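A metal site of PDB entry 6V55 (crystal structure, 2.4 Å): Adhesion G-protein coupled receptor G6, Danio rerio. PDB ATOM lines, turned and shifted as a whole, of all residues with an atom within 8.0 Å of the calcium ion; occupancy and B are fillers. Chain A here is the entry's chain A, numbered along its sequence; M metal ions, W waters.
The backbone carbonyl oxygen of Asp 98 lies within hydrogen-bond range of the backbone NH of Ser 28. OH of Tyr 25 sits at hydrogen-bond distance from N of Glu 53 (3.3 Å). The backbone NH of Val 101 lies within hydrogen-bond range of the side-chain carboxylate of Asp 526, at 3.0 Å. OD1 of Asp 98 is in salt-bridge range of NZ of Lys 477 (2.9 Å). OG of Ser 100 lies close to NZ of Lys 477, at 3.3 Å. NZ of Lys 477 lies within salt-bridge range of OE2 of Glu 53 (3.0 Å).
Water W1 lies within hydrogen-bond range of the backbone carbonyl oxygen of Asp 98 (2.6 Å) and the side-chain amide nitrogen of Gln 102 (2.6 Å).
Of the 22 residues printed, 5 come within 4 Å of the calcium ion. Along chain A the residues within 4 Å of the calcium ion span positions 53 to 101.
The calcium ion is bound by the side-chain carboxylate (OE1) of Glu 53 (2.5 Å), the backbone carbonyl oxygen (O) of Ser 100 (2.5 Å), the side-chain carboxylate (OD2) of Asp 98 (2.5 Å), the backbone carbonyl oxygen (O) of Val 101 (2.5 Å), the side-chain carboxylate (OD1) of Asp 61 (2.5 Å), water W1 (2.6 Å) and the side-chain carboxylate (OD2) of Asp 61 (2.7 Å). The calcium ion has seven donor atoms within binding distance.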
ATOM      1  N   TYR A  25      18.434  -6.331  -2.079  1.00  0.00           N
ATOM      2  CA  TYR A  25      17.453  -5.714  -1.215  1.00  0.00           C
ATOM      3  C   TYR A  25      17.098  -4.322  -1.726  1.00  0.00           C
ATOM      4  O   TYR A  25      17.850  -3.743  -2.516  1.00  0.00           O
ATOM      5  CB  TYR A  25      17.970  -5.671   0.229  1.00  0.00           C
ATOM      6  CG  TYR A  25      19.378  -5.199   0.482  1.00  0.00           C
ATOM      7  CD1 TYR A  25      19.711  -3.852   0.476  1.00  0.00           C
ATOM      8  CD2 TYR A  25      20.376  -6.103   0.838  1.00  0.00           C
ATOM      9  CE1 TYR A  25      20.994  -3.421   0.749  1.00  0.00           C
ATOM     10  CE2 TYR A  25      21.658  -5.696   1.112  1.00  0.00           C
ATOM     11  CZ  TYR A  25      21.964  -4.343   1.073  1.00  0.00           C
ATOM     12  OH  TYR A  25      23.245  -3.919   1.361  1.00  0.00           O
ATOM     13  N   PRO A  26      15.932  -3.786  -1.372  1.00  0.00           N
ATOM     14  CA  PRO A  26      15.628  -2.417  -1.776  1.00  0.00           C
ATOM     15  C   PRO A  26      16.382  -1.450  -0.877  1.00  0.00           C
ATOM     16  O   PRO A  26      16.884  -1.851   0.186  1.00  0.00           O
ATOM     17  CB  PRO A  26      14.093  -2.333  -1.593  1.00  0.00           C
ATOM     18  CG  PRO A  26      13.633  -3.772  -1.540  1.00  0.00           C
ATOM     19  CD  PRO A  26      14.729  -4.456  -0.837  1.00  0.00           C
ATOM     20  N   PRO A  27      16.528  -0.184  -1.277  1.00  0.00           N
ATOM     21  CA  PRO A  27      17.059   0.806  -0.331  1.00  0.00           C
ATOM     22  C   PRO A  27      16.075   1.119   0.783  1.00  0.00           C
ATOM     23  O   PRO A  27      14.897   0.743   0.727  1.00  0.00           O
ATOM     24  CB  PRO A  27      17.283   2.049  -1.212  1.00  0.00           C
ATOM     25  CG  PRO A  27      17.050   1.644  -2.592  1.00  0.00           C
ATOM     26  CD  PRO A  27      16.267   0.401  -2.590  1.00  0.00           C
ATOM     27  N   SER A  28      16.601   1.800   1.823  1.00  0.00           N
ATOM     28  CA  SER A  28      15.831   2.406   2.921  1.00  0.00           C
ATOM     29  C   SER A  28      14.955   1.418   3.682  1.00  0.00           C
ATOM     30  O   SER A  28      13.844   1.738   4.118  1.00  0.00           O
ATOM     31  CB  SER A  28      15.007   3.566   2.402  1.00  0.00           C
ATOM     32  OG  SER A  28      15.788   4.258   1.457  1.00  0.00           O
ATOM     33  N   LEU A  52      26.465  -7.601   2.477  1.00  0.00           N
ATOM     34  CA  LEU A  52      25.960  -6.245   2.614  1.00  0.00           C
ATOM     35  C   LEU A  52      26.969  -5.257   2.047  1.00  0.00           C
ATOM     36  O   LEU A  52      28.127  -5.612   1.782  1.00  0.00           O
ATOM     37  CB  LEU A  52      25.675  -5.901   4.077  1.00  0.00           C
ATOM     38  CG  LEU A  52      24.197  -5.887   4.481  1.00  0.00           C
ATOM     39  CD1 LEU A  52      23.626  -7.281   4.357  1.00  0.00           C
ATOM     40  CD2 LEU A  52      24.095  -5.415   5.904  1.00  0.00           C
ATOM     41  N   GLU A  53      26.512  -4.037   1.826  1.00  0.00           N
ATOM     42  CA  GLU A  53      27.387  -2.930   1.434  1.00  0.00           C
ATOM     43  C   GLU A  53      28.376  -2.654   2.565  1.00  0.00           C
ATOM     44  O   GLU A  53      27.976  -2.486   3.717  1.00  0.00           O
ATOM     45  CB  GLU A  53      26.549  -1.694   1.141  1.00  0.00           C
ATOM     46  CG  GLU A  53      27.356  -0.450   0.963  1.00  0.00           C
ATOM     47  CD  GLU A  53      26.509   0.806   0.730  1.00  0.00           C
ATOM     48  OE1 GLU A  53      25.312   0.815   1.079  1.00  0.00           O
ATOM     49  OE2 GLU A  53      27.057   1.798   0.201  1.00  0.00           O
ATOM     50  N   GLU A  54      29.668  -2.687   2.258  1.00  0.00           N
ATOM     51  CA  GLU A  54      30.649  -2.504   3.326  1.00  0.00           C
ATOM     52  C   GLU A  54      30.868  -1.023   3.621  1.00  0.00           C
ATOM     53  O   GLU A  54      30.771  -0.174   2.726  1.00  0.00           O
ATOM     54  CB  GLU A  54      31.963  -3.207   2.989  1.00  0.00           C
ATOM     55  CG  GLU A  54      32.752  -3.634   4.258  1.00  0.00           C
ATOM     56  CD  GLU A  54      34.111  -4.241   3.966  1.00  0.00           C
ATOM     57  OE1 GLU A  54      34.714  -4.835   4.898  1.00  0.00           O
ATOM     58  OE2 GLU A  54      34.557  -4.152   2.799  1.00  0.00           O
ATOM     59  N   TYR A  60      26.675   2.405   6.513  1.00  0.00           N
ATOM     60  CA  TYR A  60      25.833   2.486   5.320  1.00  0.00           C
ATOM     61  C   TYR A  60      24.681   1.483   5.439  1.00  0.00           C
ATOM     62  O   TYR A  60      23.564   1.898   5.758  1.00  0.00           O
ATOM     63  CB  TYR A  60      26.645   2.237   4.041  1.00  0.00           C
ATOM     64  CG  TYR A  60      27.625   3.344   3.679  1.00  0.00           C
ATOM     65  CD1 TYR A  60      27.550   4.592   4.270  1.00  0.00           C
ATOM     66  CD2 TYR A  60      28.625   3.130   2.715  1.00  0.00           C
ATOM     67  CE1 TYR A  60      28.450   5.593   3.942  1.00  0.00           C
ATOM     68  CE2 TYR A  60      29.516   4.127   2.391  1.00  0.00           C
ATOM     69  CZ  TYR A  60      29.425   5.348   2.999  1.00  0.00           C
ATOM     70  OH  TYR A  60      30.305   6.356   2.659  1.00  0.00           O
ATOM     71  N   ASP A  61      24.912   0.199   5.184  1.00  0.00           N
ATOM     72  CA  ASP A  61      23.937  -0.830   5.493  1.00  0.00           C
ATOM     73  C   ASP A  61      24.483  -1.686   6.616  1.00  0.00           C
ATOM     74  O   ASP A  61      25.650  -2.078   6.573  1.00  0.00           O
ATOM     75  CB  ASP A  61      23.647  -1.747   4.298  1.00  0.00           C
ATOM     76  CG  ASP A  61      23.299  -0.993   3.037  1.00  0.00           C
ATOM     77  OD1 ASP A  61      22.971   0.199   3.151  1.00  0.00           O
ATOM     78  OD2 ASP A  61      23.357  -1.592   1.927  1.00  0.00           O
ATOM     79  N   ARG A  62      23.646  -2.023   7.601  1.00  0.00           N
ATOM     80  CA  ARG A  62      24.117  -2.863   8.694  1.00  0.00           C
ATOM     81  C   ARG A  62      23.035  -3.851   9.101  1.00  0.00           C
ATOM     82  O   ARG A  62      21.846  -3.599   8.935  1.00  0.00           O
ATOM     83  CB  ARG A  62      24.557  -2.030   9.919  1.00  0.00           C
ATOM     84  CG  ARG A  62      23.455  -1.219  10.564  1.00  0.00           C
ATOM     85  CD  ARG A  62      23.894  -0.640  11.923  1.00  0.00           C
ATOM     86  NE  ARG A  62      25.039   0.274  11.805  1.00  0.00           N
ATOM     87  CZ  ARG A  62      25.376   1.192  12.707  1.00  0.00           C
ATOM     88  NH1 ARG A  62      24.668   1.372  13.823  1.00  0.00           N
ATOM     89  NH2 ARG A  62      26.439   1.965  12.460  1.00  0.00           N
ATOM     90  N   PHE A  95      17.805  -5.093  10.352  1.00  0.00           N
ATOM     91  CA  PHE A  95      18.489  -4.798   9.106  1.00  0.00           C
ATOM     92  C   PHE A  95      18.044  -3.430   8.634  1.00  0.00           C
ATOM     93  O   PHE A  95      16.843  -3.146   8.589  1.00  0.00           O
ATOM     94  CB  PHE A  95      18.210  -5.862   8.043  1.00  0.00           C
ATOM     95  CG  PHE A  95      18.652  -5.494   6.638  1.00  0.00           C
ATOM     96  CD1 PHE A  95      19.979  -5.145   6.365  1.00  0.00           C
ATOM     97  CD2 PHE A  95      17.746  -5.513   5.587  1.00  0.00           C
ATOM     98  CE1 PHE A  95      20.383  -4.824   5.048  1.00  0.00           C
ATOM     99  CE2 PHE A  95      18.146  -5.203   4.277  1.00  0.00           C
ATOM    100  CZ  PHE A  95      19.473  -4.855   4.004  1.00  0.00           C
ATOM    101  N   ASN A  96      19.016  -2.575   8.302  1.00  0.00           N
ATOM    102  CA  ASN A  96      18.767  -1.222   7.783  1.00  0.00           C
ATOM    103  C   ASN A  96      19.662  -0.965   6.590  1.00  0.00           C
ATOM    104  O   ASN A  96      20.875  -1.236   6.649  1.00  0.00           O
ATOM    105  CB  ASN A  96      19.009  -0.180   8.875  1.00  0.00           C
ATOM    106  CG  ASN A  96      18.045  -0.309  10.000  1.00  0.00           C
ATOM    107  OD1 ASN A  96      16.848  -0.014   9.858  1.00  0.00           O
ATOM    108  ND2 ASN A  96      18.531  -0.758  11.147  1.00  0.00           N
ATOM    109  N   SER A  97      19.080  -0.491   5.491  1.00  0.00           N
ATOM    110  CA  SER A  97      19.855  -0.123   4.318  1.00  0.00           C
ATOM    111  C   SER A  97      19.672   1.370   4.125  1.00  0.00           C
ATOM    112  O   SER A  97      18.655   1.934   4.566  1.00  0.00           O
ATOM    113  CB  SER A  97      19.402  -0.856   3.053  1.00  0.00           C
ATOM    114  OG  SER A  97      17.989  -0.724   2.918  1.00  0.00           O
ATOM    115  N   ASP A  98      20.612   2.031   3.467  1.00  0.00           N
ATOM    116  CA  ASP A  98      20.413   3.451   3.269  1.00  0.00           C
ATOM    117  C   ASP A  98      19.842   3.653   1.866  1.00  0.00           C
ATOM    118  O   ASP A  98      19.229   2.738   1.327  1.00  0.00           O
ATOM    119  CB  ASP A  98      21.704   4.251   3.553  1.00  0.00           C
ATOM    120  CG  ASP A  98      22.924   3.823   2.712  1.00  0.00           C
ATOM    121  OD1 ASP A  98      24.034   4.270   3.061  1.00  0.00           O
ATOM    122  OD2 ASP A  98      22.832   3.106   1.710  1.00  0.00           O
ATOM    123  N   PHE A  99      20.052   4.836   1.270  1.00  0.00           N
ATOM    124  CA  PHE A  99      19.398   5.270   0.032  1.00  0.00           C
ATOM    125  C   PHE A  99      20.064   4.775  -1.243  1.00  0.00           C
ATOM    126  O   PHE A  99      19.468   4.932  -2.311  1.00  0.00           O
ATOM    127  CB  PHE A  99      19.325   6.806  -0.041  1.00  0.00           C
ATOM    128  CG  PHE A  99      20.622   7.511   0.303  1.00  0.00           C
ATOM    129  CD1 PHE A  99      21.570   7.775  -0.685  1.00  0.00           C
ATOM    130  CD2 PHE A  99      20.890   7.927   1.604  1.00  0.00           C
ATOM    131  CE1 PHE A  99      22.778   8.410  -0.382  1.00  0.00           C
ATOM    132  CE2 PHE A  99      22.093   8.550   1.914  1.00  0.00           C
ATOM    133  CZ  PHE A  99      23.033   8.789   0.906  1.00  0.00           C
ATOM    134  N   SER A 100      21.272   4.213  -1.191  1.00  0.00           N
ATOM    135  CA  SER A 100      21.969   3.862  -2.432  1.00  0.00           C
ATOM    136  C   SER A 100      22.946   2.732  -2.171  1.00  0.00           C
ATOM    137  O   SER A 100      23.338   2.497  -1.030  1.00  0.00           O
ATOM    138  CB  SER A 100      22.726   5.059  -3.000  1.00  0.00           C
ATOM    139  OG  SER A 100      23.907   5.232  -2.233  1.00  0.00           O
ATOM    140  N   VAL A 101      23.366   2.056  -3.266  1.00  0.00           N
ATOM    141  CA  VAL A 101      24.266   0.889  -3.304  1.00  0.00           C
ATOM    142  C   VAL A 101      23.688  -0.304  -2.540  1.00  0.00           C
ATOM    143  O   VAL A 101      23.785  -0.368  -1.314  1.00  0.00           O
ATOM    144  CB  VAL A 101      25.693   1.196  -2.797  1.00  0.00           C
ATOM    145  CG1 VAL A 101      26.616   0.027  -3.019  1.00  0.00           C
ATOM    146  CG2 VAL A 101      26.243   2.464  -3.435  1.00  0.00           C
ATOM    147  N   GLN A 102      23.158  -1.286  -3.263  1.00  0.00           N
ATOM    148  CA  GLN A 102      22.557  -2.460  -2.654  1.00  0.00           C
ATOM    149  C   GLN A 102      23.299  -3.712  -3.078  1.00  0.00           C
ATOM    150  O   GLN A 102      23.728  -3.834  -4.224  1.00  0.00           O
ATOM    151  CB  GLN A 102      21.096  -2.570  -3.031  1.00  0.00           C
ATOM    152  CG  GLN A 102      20.258  -1.563  -2.292  1.00  0.00           C
ATOM    153  CD  GLN A 102      20.098  -0.289  -3.058  1.00  0.00           C
ATOM    154  OE1 GLN A 102      19.823  -0.313  -4.244  1.00  0.00           O
ATOM    155  NE2 GLN A 102      20.295   0.836  -2.379  1.00  0.00           N
ATOM    156  N   LYS A 103      23.477  -4.628  -2.137  1.00  0.00           N
ATOM    157  CA  LYS A 103      24.022  -5.933  -2.410  1.00  0.00           C
ATOM    158  C   LYS A 103      22.942  -6.987  -2.162  1.00  0.00           C
ATOM    159  O   LYS A 103      21.750  -6.672  -2.030  1.00  0.00           O
ATOM    160  CB  LYS A 103      25.259  -6.181  -1.547  1.00  0.00           C
ATOM    161  CG  LYS A 103      26.339  -5.125  -1.705  1.00  0.00           C
ATOM    162  CD  LYS A 103      26.977  -5.115  -3.091  1.00  0.00           C
ATOM    163  CE  LYS A 103      27.692  -3.786  -3.321  1.00  0.00           C
ATOM    164  NZ  LYS A 103      28.927  -3.893  -4.128  1.00  0.00           N
ATOM    165  N   PRO A 472      25.794   8.629   5.899  1.00  0.00           N
ATOM    166  CA  PRO A 472      26.253   9.236   4.652  1.00  0.00           C
ATOM    167  C   PRO A 472      25.530  10.505   4.277  1.00  0.00           C
ATOM    168  O   PRO A 472      24.333  10.673   4.532  1.00  0.00           O
ATOM    169  CB  PRO A 472      25.972   8.145   3.615  1.00  0.00           C
ATOM    170  CG  PRO A 472      25.026   7.213   4.256  1.00  0.00           C
ATOM    171  CD  PRO A 472      25.481   7.202   5.659  1.00  0.00           C
ATOM    172  N   LYS A 477      27.512  10.593  -0.801  1.00  0.00           N
ATOM    173  CA  LYS A 477      28.173   9.765   0.231  1.00  0.00           C
ATOM    174  C   LYS A 477      29.691   9.933   0.284  1.00  0.00           C
ATOM    175  O   LYS A 477      30.383   9.053   0.802  1.00  0.00           O
ATOM    176  CB  LYS A 477      27.861   8.275   0.104  1.00  0.00           C
ATOM    177  CG  LYS A 477      26.423   7.874  -0.057  1.00  0.00           C
ATOM    178  CD  LYS A 477      26.379   6.381  -0.420  1.00  0.00           C
ATOM    179  CE  LYS A 477      26.289   5.465   0.780  1.00  0.00           C
ATOM    180  NZ  LYS A 477      25.423   4.281   0.515  1.00  0.00           N
ATOM    181  N   ASP A 526      21.342   5.639  -8.892  1.00  0.00           N
ATOM    182  CA  ASP A 526      20.870   4.849  -7.764  1.00  0.00           C
ATOM    183  C   ASP A 526      19.561   5.386  -7.182  1.00  0.00           C
ATOM    184  O   ASP A 526      18.614   4.603  -7.005  1.00  0.00           O
ATOM    185  CB  ASP A 526      21.963   4.781  -6.686  1.00  0.00           C
ATOM    186  CG  ASP A 526      22.149   3.375  -6.118  1.00  0.00           C
ATOM    187  OD1 ASP A 526      23.307   2.887  -6.142  1.00  0.00           O
ATOM    188  OD2 ASP A 526      21.165   2.757  -5.646  1.00  0.00           O
HETATM  189 CA    CA M   1      22.884   0.816   0.711  1.00  0.00          CA
HETATM  190  O   HOH W   1      20.371   0.670   0.261  1.00  0.00           O
